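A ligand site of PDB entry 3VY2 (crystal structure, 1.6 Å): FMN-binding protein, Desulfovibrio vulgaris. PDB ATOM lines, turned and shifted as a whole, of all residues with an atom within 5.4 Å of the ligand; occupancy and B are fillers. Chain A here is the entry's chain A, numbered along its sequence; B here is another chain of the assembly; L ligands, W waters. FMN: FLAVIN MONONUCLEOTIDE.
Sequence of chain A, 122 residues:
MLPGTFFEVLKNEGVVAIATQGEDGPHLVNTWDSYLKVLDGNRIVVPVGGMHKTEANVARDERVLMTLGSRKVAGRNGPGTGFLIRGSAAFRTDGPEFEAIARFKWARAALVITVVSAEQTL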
ATOM      1  N   VAL A  15      28.748   7.999  -5.805  1.00  0.00           N
ATOM      2  CA  VAL A  15      29.386   6.750  -5.412  1.00  0.00           C
ATOM      3  C   VAL A  15      30.440   7.041  -4.350  1.00  0.00           C
ATOM      4  O   VAL A  15      31.317   7.877  -4.546  1.00  0.00           O
ATOM      5  CB  VAL A  15      30.032   6.072  -6.635  1.00  0.00           C
ATOM      6  CG1 VAL A  15      30.803   4.829  -6.215  1.00  0.00           C
ATOM      7  CG2 VAL A  15      28.945   5.708  -7.654  1.00  0.00           C
ATOM      8  N   HIS A  27      42.025  -3.284  -0.827  1.00  0.00           N
ATOM      9  CA  HIS A  27      40.724  -3.666  -1.370  1.00  0.00           C
ATOM     10  C   HIS A  27      39.880  -2.404  -1.431  1.00  0.00           C
ATOM     11  O   HIS A  27      40.135  -1.459  -0.693  1.00  0.00           O
ATOM     12  CB  HIS A  27      40.048  -4.751  -0.530  1.00  0.00           C
ATOM     13  CG  HIS A  27      38.843  -5.348  -1.198  1.00  0.00           C
ATOM     14  ND1 HIS A  27      38.844  -5.756  -2.508  1.00  0.00           N
ATOM     15  CD2 HIS A  27      37.588  -5.577  -0.730  1.00  0.00           C
ATOM     16  CE1 HIS A  27      37.647  -6.227  -2.832  1.00  0.00           C
ATOM     17  NE2 HIS A  27      36.869  -6.141  -1.762  1.00  0.00           N
ATOM     18  N   VAL A  29      35.734  -1.086  -2.098  1.00  0.00           N
ATOM     19  CA  VAL A  29      34.302  -1.360  -2.277  1.00  0.00           C
ATOM     20  C   VAL A  29      33.514  -0.046  -2.240  1.00  0.00           C
ATOM     21  O   VAL A  29      34.082   1.024  -1.999  1.00  0.00           O
ATOM     22  CB  VAL A  29      33.744  -2.327  -1.214  1.00  0.00           C
ATOM     23  CG1 VAL A  29      34.441  -3.686  -1.289  1.00  0.00           C
ATOM     24  CG2 VAL A  29      33.832  -1.723   0.206  1.00  0.00           C
ATOM     25  N   ASN A  30      32.209  -0.140  -2.467  1.00  0.00           N
ATOM     26  CA  ASN A  30      31.392   1.050  -2.634  1.00  0.00           C
ATOM     27  C   ASN A  30      30.127   1.053  -1.816  1.00  0.00           C
ATOM     28  O   ASN A  30      29.641   0.007  -1.382  1.00  0.00           O
ATOM     29  CB  ASN A  30      31.014   1.227  -4.107  1.00  0.00           C
ATOM     30  CG  ASN A  30      32.211   1.385  -5.003  1.00  0.00           C
ATOM     31  OD1 ASN A  30      32.527   0.506  -5.808  1.00  0.00           O
ATOM     32  ND2 ASN A  30      32.919   2.501  -4.843  1.00  0.00           N
ATOM     33  N   THR A  31      29.610   2.256  -1.600  1.00  0.00           N
ATOM     34  CA  THR A  31      28.213   2.458  -1.243  1.00  0.00           C
ATOM     35  C   THR A  31      27.708   3.715  -1.963  1.00  0.00           C
ATOM     36  O   THR A  31      28.399   4.261  -2.832  1.00  0.00           O
ATOM     37  CB  THR A  31      27.981   2.447   0.301  1.00  0.00           C
ATOM     38  OG1 THR A  31      26.579   2.426   0.577  1.00  0.00           O
ATOM     39  CG2 THR A  31      28.611   3.659   0.965  1.00  0.00           C
ATOM     40  N   TRP A  32      26.490   4.138  -1.649  1.00  0.00           N
ATOM     41  CA  TRP A  32      25.918   5.352  -2.215  1.00  0.00           C
ATOM     42  C   TRP A  32      25.932   6.496  -1.212  1.00  0.00           C
ATOM     43  O   TRP A  32      25.804   6.270  -0.010  1.00  0.00           O
ATOM     44  CB  TRP A  32      24.460   5.103  -2.616  1.00  0.00           C
ATOM     45  CG  TRP A  32      24.271   4.075  -3.685  1.00  0.00           C
ATOM     46  CD1 TRP A  32      23.796   2.807  -3.521  1.00  0.00           C
ATOM     47  CD2 TRP A  32      24.512   4.240  -5.086  1.00  0.00           C
ATOM     48  NE1 TRP A  32      23.744   2.156  -4.727  1.00  0.00           N
ATOM     49  CE2 TRP A  32      24.167   3.021  -5.707  1.00  0.00           C
ATOM     50  CE3 TRP A  32      24.986   5.302  -5.872  1.00  0.00           C
ATOM     51  CZ2 TRP A  32      24.287   2.828  -7.088  1.00  0.00           C
ATOM     52  CZ3 TRP A  32      25.107   5.095  -7.252  1.00  0.00           C
ATOM     53  CH2 TRP A  32      24.752   3.876  -7.841  1.00  0.00           C
ATOM     54  N   TYR A  35      23.090   6.429   1.183  1.00  0.00           N
ATOM     55  CA  TYR A  35      23.044   5.350   2.177  1.00  0.00           C
ATOM     56  C   TYR A  35      23.785   5.698   3.468  1.00  0.00           C
ATOM     57  O   TYR A  35      23.558   5.081   4.508  1.00  0.00           O
ATOM     58  CB  TYR A  35      23.664   4.060   1.612  1.00  0.00           C
ATOM     59  CG  TYR A  35      22.811   3.271   0.632  1.00  0.00           C
ATOM     60  CD1 TYR A  35      21.685   3.820   0.019  1.00  0.00           C
ATOM     61  CD2 TYR A  35      23.175   1.972   0.297  1.00  0.00           C
ATOM     62  CE1 TYR A  35      20.931   3.079  -0.896  1.00  0.00           C
ATOM     63  CE2 TYR A  35      22.424   1.224  -0.611  1.00  0.00           C
ATOM     64  CZ  TYR A  35      21.304   1.789  -1.198  1.00  0.00           C
ATOM     65  OH  TYR A  35      20.567   1.042  -2.096  1.00  0.00           O
ATOM     66  N   VAL A  46      27.509   2.711   7.334  1.00  0.00           N
ATOM     67  CA  VAL A  46      27.217   2.162   6.014  1.00  0.00           C
ATOM     68  C   VAL A  46      26.429   0.851   6.169  1.00  0.00           C
ATOM     69  O   VAL A  46      26.839  -0.007   6.959  1.00  0.00           O
ATOM     70  CB  VAL A  46      28.527   1.839   5.262  1.00  0.00           C
ATOM     71  CG1 VAL A  46      28.261   1.247   3.879  1.00  0.00           C
ATOM     72  CG2 VAL A  46      29.414   3.075   5.142  1.00  0.00           C
ATOM     73  N   PRO A  47      25.304   0.700   5.436  1.00  0.00           N
ATOM     74  CA  PRO A  47      24.619  -0.607   5.443  1.00  0.00           C
ATOM     75  C   PRO A  47      25.459  -1.684   4.727  1.00  0.00           C
ATOM     76  O   PRO A  47      25.950  -1.449   3.625  1.00  0.00           O
ATOM     77  CB  PRO A  47      23.316  -0.321   4.691  1.00  0.00           C
ATOM     78  CG  PRO A  47      23.625   0.849   3.799  1.00  0.00           C
ATOM     79  CD  PRO A  47      24.631   1.687   4.568  1.00  0.00           C
ATOM     80  N   VAL A  48      25.621  -2.833   5.378  1.00  0.00           N
ATOM     81  CA  VAL A  48      26.442  -3.919   4.844  1.00  0.00           C
ATOM     82  C   VAL A  48      25.586  -5.068   4.353  1.00  0.00           C
ATOM     83  O   VAL A  48      24.898  -5.723   5.132  1.00  0.00           O
ATOM     84  CB  VAL A  48      27.467  -4.434   5.899  1.00  0.00           C
ATOM     85  CG1 VAL A  48      28.241  -5.637   5.386  1.00  0.00           C
ATOM     86  CG2 VAL A  48      28.438  -3.314   6.277  1.00  0.00           C
ATOM     87  N   GLY A  49      25.624  -5.302   3.036  1.00  0.00           N
ATOM     88  CA  GLY A  49      25.031  -6.493   2.433  1.00  0.00           C
ATOM     89  C   GLY A  49      26.113  -7.531   2.190  1.00  0.00           C
ATOM     90  O   GLY A  49      26.034  -8.664   2.704  1.00  0.00           O
ATOM     91  N   GLY A  50      27.118  -7.151   1.417  1.00  0.00           N
ATOM     92  CA  GLY A  50      28.259  -8.021   1.139  1.00  0.00           C
ATOM     93  C   GLY A  50      29.405  -7.684   2.068  1.00  0.00           C
ATOM     94  O   GLY A  50      29.366  -8.030   3.252  1.00  0.00           O
ATOM     95  N   MET A  51      30.412  -7.019   1.520  1.00  0.00           N
ATOM     96  CA  MET A  51      31.597  -6.549   2.261  1.00  0.00           C
ATOM     97  C   MET A  51      32.256  -7.638   3.124  1.00  0.00           C
ATOM     98  O   MET A  51      32.685  -7.388   4.253  1.00  0.00           O
ATOM     99  CB  MET A  51      31.269  -5.287   3.060  1.00  0.00           C
ATOM    100  CG  MET A  51      30.786  -4.133   2.178  1.00  0.00           C
ATOM    101  SD  MET A  51      30.890  -2.559   3.039  1.00  0.00           S
ATOM    102  CE  MET A  51      30.287  -1.458   1.767  1.00  0.00           C
ATOM    103  N   HIS A  52      32.339  -8.843   2.570  1.00  0.00           N
ATOM    104  CA  HIS A  52      32.952  -9.977   3.265  1.00  0.00           C
ATOM    105  C   HIS A  52      34.464  -9.878   3.277  1.00  0.00           C
ATOM    106  O   HIS A  52      35.103 -10.096   4.314  1.00  0.00           O
ATOM    107  CB  HIS A  52      32.471 -11.286   2.653  1.00  0.00           C
ATOM    108  CG  HIS A  52      30.999 -11.524   2.808  1.00  0.00           C
ATOM    109  ND1 HIS A  52      30.431 -11.862   4.012  1.00  0.00           N
ATOM    110  CD2 HIS A  52      29.985 -11.436   1.917  1.00  0.00           C
ATOM    111  CE1 HIS A  52      29.119 -11.990   3.856  1.00  0.00           C
ATOM    112  NE2 HIS A  52      28.827 -11.727   2.589  1.00  0.00           N
ATOM    113  N   LYS A  53      35.059  -9.550   2.125  1.00  0.00           N
ATOM    114  CA  LYS A  53      36.496  -9.319   2.061  1.00  0.00           C
ATOM    115  C   LYS A  53      36.859  -8.084   2.890  1.00  0.00           C
ATOM    116  O   LYS A  53      37.822  -8.103   3.666  1.00  0.00           O
ATOM    117  CB  LYS A  53      36.952  -9.193   0.600  1.00  0.00           C
ATOM    118  CG  LYS A  53      38.442  -8.917   0.445  1.00  0.00           C
ATOM    119  CD  LYS A  53      39.104  -9.767  -0.632  1.00  0.00           C
ATOM    120  CE  LYS A  53      38.547  -9.533  -2.026  1.00  0.00           C
ATOM    121  NZ  LYS A  53      37.454 -10.493  -2.380  1.00  0.00           N
ATOM    122  N   THR A  54      36.085  -7.018   2.732  1.00  0.00           N
ATOM    123  CA  THR A  54      36.224  -5.791   3.509  1.00  0.00           C
ATOM    124  C   THR A  54      36.192  -6.076   5.018  1.00  0.00           C
ATOM    125  O   THR A  54      37.051  -5.587   5.756  1.00  0.00           O
ATOM    126  CB  THR A  54      35.149  -4.769   3.094  1.00  0.00           C
ATOM    127  OG1 THR A  54      35.349  -4.436   1.710  1.00  0.00           O
ATOM    128  CG2 THR A  54      35.215  -3.483   3.925  1.00  0.00           C
ATOM    129  N   GLU A  55      35.230  -6.875   5.466  1.00  0.00           N
ATOM    130  CA  GLU A  55      35.146  -7.231   6.884  1.00  0.00           C
ATOM    131  C   GLU A  55      36.378  -7.995   7.370  1.00  0.00           C
ATOM    132  O   GLU A  55      36.906  -7.724   8.453  1.00  0.00           O
ATOM    133  CB  GLU A  55      33.873  -8.014   7.207  1.00  0.00           C
ATOM    134  CG  GLU A  55      33.717  -8.261   8.698  1.00  0.00           C
ATOM    135  CD  GLU A  55      32.425  -8.928   9.094  1.00  0.00           C
ATOM    136  OE1 GLU A  55      31.629  -9.310   8.205  1.00  0.00           O
ATOM    137  OE2 GLU A  55      32.202  -9.063  10.318  1.00  0.00           O
ATOM    138  N   TRP A 106      18.158  -5.767   3.695  1.00  0.00           N
ATOM    139  CA  TRP A 106      19.214  -6.632   3.168  1.00  0.00           C
ATOM    140  C   TRP A 106      20.511  -6.512   3.979  1.00  0.00           C
ATOM    141  O   TRP A 106      21.465  -7.263   3.740  1.00  0.00           O
ATOM    142  CB  TRP A 106      19.470  -6.304   1.687  1.00  0.00           C
ATOM    143  CG  TRP A 106      19.610  -4.831   1.370  1.00  0.00           C
ATOM    144  CD1 TRP A 106      18.636  -4.001   0.894  1.00  0.00           C
ATOM    145  CD2 TRP A 106      20.790  -4.027   1.516  1.00  0.00           C
ATOM    146  NE1 TRP A 106      19.139  -2.730   0.721  1.00  0.00           N
ATOM    147  CE2 TRP A 106      20.465  -2.722   1.102  1.00  0.00           C
ATOM    148  CE3 TRP A 106      22.099  -4.296   1.941  1.00  0.00           C
ATOM    149  CZ2 TRP A 106      21.392  -1.676   1.100  1.00  0.00           C
ATOM    150  CZ3 TRP A 106      23.028  -3.243   1.945  1.00  0.00           C
ATOM    151  CH2 TRP A 106      22.670  -1.962   1.520  1.00  0.00           C
ATOM    152  N   LEU B  68      33.915   2.960  -9.867  1.00  0.00           N
ATOM    153  CA  LEU B  68      33.079   4.028 -10.413  1.00  0.00           C
ATOM    154  C   LEU B  68      31.688   3.460 -10.571  1.00  0.00           C
ATOM    155  O   LEU B  68      31.505   2.249 -10.576  1.00  0.00           O
ATOM    156  CB  LEU B  68      33.623   4.523 -11.760  1.00  0.00           C
ATOM    157  CG  LEU B  68      33.512   3.610 -12.992  1.00  0.00           C
ATOM    158  CD1 LEU B  68      33.770   4.421 -14.260  1.00  0.00           C
ATOM    159  CD2 LEU B  68      34.453   2.414 -12.904  1.00  0.00           C
ATOM    160  N   GLY B  69      30.703   4.338 -10.685  1.00  0.00           N
ATOM    161  CA  GLY B  69      29.326   3.871 -10.838  1.00  0.00           C
ATOM    162  C   GLY B  69      28.376   5.008 -11.149  1.00  0.00           C
ATOM    163  O   GLY B  69      28.784   6.168 -11.177  1.00  0.00           O
ATOM    164  N   THR B  81      24.402   1.069 -10.797  1.00  0.00           N
ATOM    165  CA  THR B  81      25.405   0.029 -10.914  1.00  0.00           C
ATOM    166  C   THR B  81      26.795   0.624 -10.787  1.00  0.00           C
ATOM    167  O   THR B  81      26.947   1.848 -10.745  1.00  0.00           O
ATOM    168  CB  THR B  81      25.275  -0.754 -12.244  1.00  0.00           C
ATOM    169  OG1 THR B  81      26.099  -1.927 -12.190  1.00  0.00           O
ATOM    170  CG2 THR B  81      25.688   0.088 -13.442  1.00  0.00           C
ATOM    171  N   GLY B  82      27.798  -0.241 -10.752  1.00  0.00           N
ATOM    172  CA  GLY B  82      29.170   0.202 -10.692  1.00  0.00           C
ATOM    173  C   GLY B  82      30.119  -0.947 -10.919  1.00  0.00           C
ATOM    174  O   GLY B  82      29.676  -2.096 -11.111  1.00  0.00           O
ATOM    175  N   PHE B  83      31.411  -0.641 -10.886  1.00  0.00           N
ATOM    176  CA  PHE B  83      32.477  -1.578 -11.257  1.00  0.00           C
ATOM    177  C   PHE B  83      33.673  -1.513 -10.347  1.00  0.00           C
ATOM    178  O   PHE B  83      34.036  -0.446  -9.847  1.00  0.00           O
ATOM    179  CB  PHE B  83      32.942  -1.286 -12.679  1.00  0.00           C
ATOM    180  CG  PHE B  83      31.958  -1.704 -13.717  1.00  0.00           C
ATOM    181  CD1 PHE B  83      30.923  -0.841 -14.111  1.00  0.00           C
ATOM    182  CD2 PHE B  83      32.031  -2.975 -14.287  1.00  0.00           C
ATOM    183  CE1 PHE B  83      29.979  -1.260 -15.050  1.00  0.00           C
ATOM    184  CE2 PHE B  83      31.096  -3.393 -15.228  1.00  0.00           C
ATOM    185  CZ  PHE B  83      30.077  -2.535 -15.604  1.00  0.00           C
ATOM    186  N   THR B 121      29.754  -4.846  -9.886  1.00  0.00           N
ATOM    187  CA  THR B 121      29.551  -5.243  -8.490  1.00  0.00           C
ATOM    188  C   THR B 121      28.154  -4.936  -7.962  1.00  0.00           C
ATOM    189  O   THR B 121      27.884  -5.104  -6.767  1.00  0.00           O
ATOM    190  CB  THR B 121      30.608  -4.588  -7.598  1.00  0.00           C
ATOM    191  OG1 THR B 121      30.606  -3.176  -7.847  1.00  0.00           O
ATOM    192  CG2 THR B 121      31.993  -5.159  -7.885  1.00  0.00           C
ATOM    193  N   LEU B 122      27.268  -4.495  -8.853  1.00  0.00           N
ATOM    194  CA  LEU B 122      25.886  -4.170  -8.486  1.00  0.00           C
ATOM    195  C   LEU B 122      24.943  -4.370  -9.675  1.00  0.00           C
ATOM    196  O   LEU B 122      25.305  -4.092 -10.815  1.00  0.00           O
ATOM    197  CB  LEU B 122      25.816  -2.723  -7.964  1.00  0.00           C
ATOM    198  CG  LEU B 122      24.471  -2.212  -7.450  1.00  0.00           C
ATOM    199  CD1 LEU B 122      24.019  -3.022  -6.236  1.00  0.00           C
ATOM    200  CD2 LEU B 122      24.614  -0.744  -7.088  1.00  0.00           C
ATOM    201  OXT LEU B 122      23.803  -4.826  -9.521  1.00  0.00           O
HETATM  202  N1  FMN L   1      27.674  -3.441  -0.862  1.00  0.00           N
HETATM  203  C2  FMN L   1      27.205  -3.347   0.441  1.00  0.00           C
HETATM  204  O2  FMN L   1      27.421  -4.266   1.232  1.00  0.00           O
HETATM  205  N3  FMN L   1      26.492  -2.219   0.859  1.00  0.00           N
HETATM  206  C4  FMN L   1      26.233  -1.180  -0.044  1.00  0.00           C
HETATM  207  O4  FMN L   1      25.606  -0.188   0.343  1.00  0.00           O
HETATM  208  C4A FMN L   1      26.712  -1.274  -1.351  1.00  0.00           C
HETATM  209  N5  FMN L   1      26.461  -0.241  -2.263  1.00  0.00           N
HETATM  210  C5A FMN L   1      27.112  -0.245  -3.493  1.00  0.00           C
HETATM  211  C6  FMN L   1      27.029   0.885  -4.306  1.00  0.00           C
HETATM  212  C7  FMN L   1      27.668   0.909  -5.533  1.00  0.00           C
HETATM  213  C7M FMN L   1      27.575   2.156  -6.417  1.00  0.00           C
HETATM  214  C8  FMN L   1      28.390  -0.218  -5.954  1.00  0.00           C
HETATM  215  C8M FMN L   1      29.089  -0.229  -7.307  1.00  0.00           C
HETATM  216  C9  FMN L   1      28.469  -1.349  -5.155  1.00  0.00           C
HETATM  217  C9A FMN L   1      27.824  -1.373  -3.911  1.00  0.00           C
HETATM  218  N10 FMN L   1      27.917  -2.493  -3.064  1.00  0.00           N
HETATM  219  C10 FMN L   1      27.415  -2.402  -1.766  1.00  0.00           C
HETATM  220  C1' FMN L   1      28.764  -3.656  -3.424  1.00  0.00           C
HETATM  221  C2' FMN L   1      30.164  -3.531  -2.761  1.00  0.00           C
HETATM  222  O2' FMN L   1      30.930  -2.494  -3.380  1.00  0.00           O
HETATM  223  C3' FMN L   1      30.968  -4.836  -2.812  1.00  0.00           C
HETATM  224  O3' FMN L   1      31.211  -5.188  -4.174  1.00  0.00           O
HETATM  225  C4' FMN L   1      30.291  -5.989  -2.064  1.00  0.00           C
HETATM  226  O4' FMN L   1      29.754  -5.527  -0.815  1.00  0.00           O
HETATM  227  C5' FMN L   1      31.283  -7.109  -1.782  1.00  0.00           C
HETATM  228  O5' FMN L   1      32.284  -6.615  -0.879  1.00  0.00           O
HETATM  229  P   FMN L   1      33.678  -7.379  -0.625  1.00  0.00           P
HETATM  230  O1P FMN L   1      34.461  -7.412  -2.016  1.00  0.00           O
HETATM  231  O2P FMN L   1      33.332  -8.918  -0.208  1.00  0.00           O
HETATM  232  O3P FMN L   1      34.416  -6.663   0.444  1.00  0.00           O
HETATM  233  O   HOH W   1      35.203  -9.337  -3.582  1.00  0.00           O
HETATM  234  O   HOH W   2      32.107  -2.193  -5.859  1.00  0.00           O
HETATM  235  O   HOH W   3      29.492  -7.202  -5.386  1.00  0.00           O
HETATM  236  O   HOH W   4      33.790  -6.182  -4.294  1.00  0.00           O
HETATM  237  O   HOH W   5      26.895  -6.788  -2.273  1.00  0.00           O
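The backbone carbonyl oxygen (O) of Pro 47 lies within hydrogen-bond range of a nitrogen (N3) of the ligand (2.9 Å).
The backbone NH of Gly 49 sits at hydrogen-bond distance from an oxygen (O2) of the ligand (2.7 Å).
The backbone NH (N) of Met 51 lies within hydrogen-bond range of an oxygen (O4') of the ligand (2.8 Å).
O1P of the ligand lies within hydrogen-bond range of NE2 of His 27, 2.7 Å away.
N of Gly 50 sits at hydrogen-bond distance from O2 of the ligand (2.9 Å).
The backbone NH (N) of His 52 sits at hydrogen-bond distance from an oxygen (O2P) of the ligand, 3.0 Å away.
The backbone NH (N) of Asn 30 lies within hydrogen-bond range of an oxygen (O2') of the ligand, 2.8 Å away.
The backbone carbonyl oxygen (O) of Asn 30 lies close to an oxygen (O2') of the ligand (3.5 Å).
The side-chain hydroxyl (OG1) of Thr 54 lies within hydrogen-bond range of an oxygen (O3P) of the ligand (2.7 Å).
N of Lys 53 sits at hydrogen-bond distance from O2P of the ligand.
The side-chain hydroxyl (OG1) of Thr 31 lies within hydrogen-bond range of an oxygen (O4) of the ligand.
The backbone NH of Thr 54 sits at hydrogen-bond distance from an oxygen (O3P) of the ligand (2.9 Å).
OG1 of Thr 81 of chain B lies within hydrogen-bond range of O of Leu 122 of chain B (2.7 Å).
O of Gly 82 of chain B lies within hydrogen-bond range of N of Thr 121 of chain B (3.0 Å).
Val 29 touches the ligand.
Trp 32 touches the ligand.
Tyr 35 touches the ligand.
Val 48 touches the ligand.
Trp 106 touches the ligand (CH2 to O4, 3.6 Å).
Gly 82 of chain B touches the ligand.
Thr 121 of chain B touches the ligand (OG1 to C8M, 3.4 Å).
Leu 122 of chain B touches the ligand (CD2 to C7, 3.8 Å).
Hydrophobic or aromatic side chains within 4 Å of the ligand: His 27, Val 29, Trp 32, Tyr 35, Met 51, His 52, Trp 106 and Leu 122 of chain B.
Water W1 lies within hydrogen-bond range of O1P of the ligand (2.6 Å) and NZ of Lys 53 (2.8 Å).
Water W2 lies within hydrogen-bond range of OG1 of Thr 121 of chain B (2.7 Å), OD1 of Asn 30 (2.7 Å) and O2' of the ligand (2.8 Å).
Water W3 lies within hydrogen-bond range of an oxygen (O3') of the ligand (2.9 Å) and the backbone carbonyl oxygen of Thr 121 of chain B (3.0 Å).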
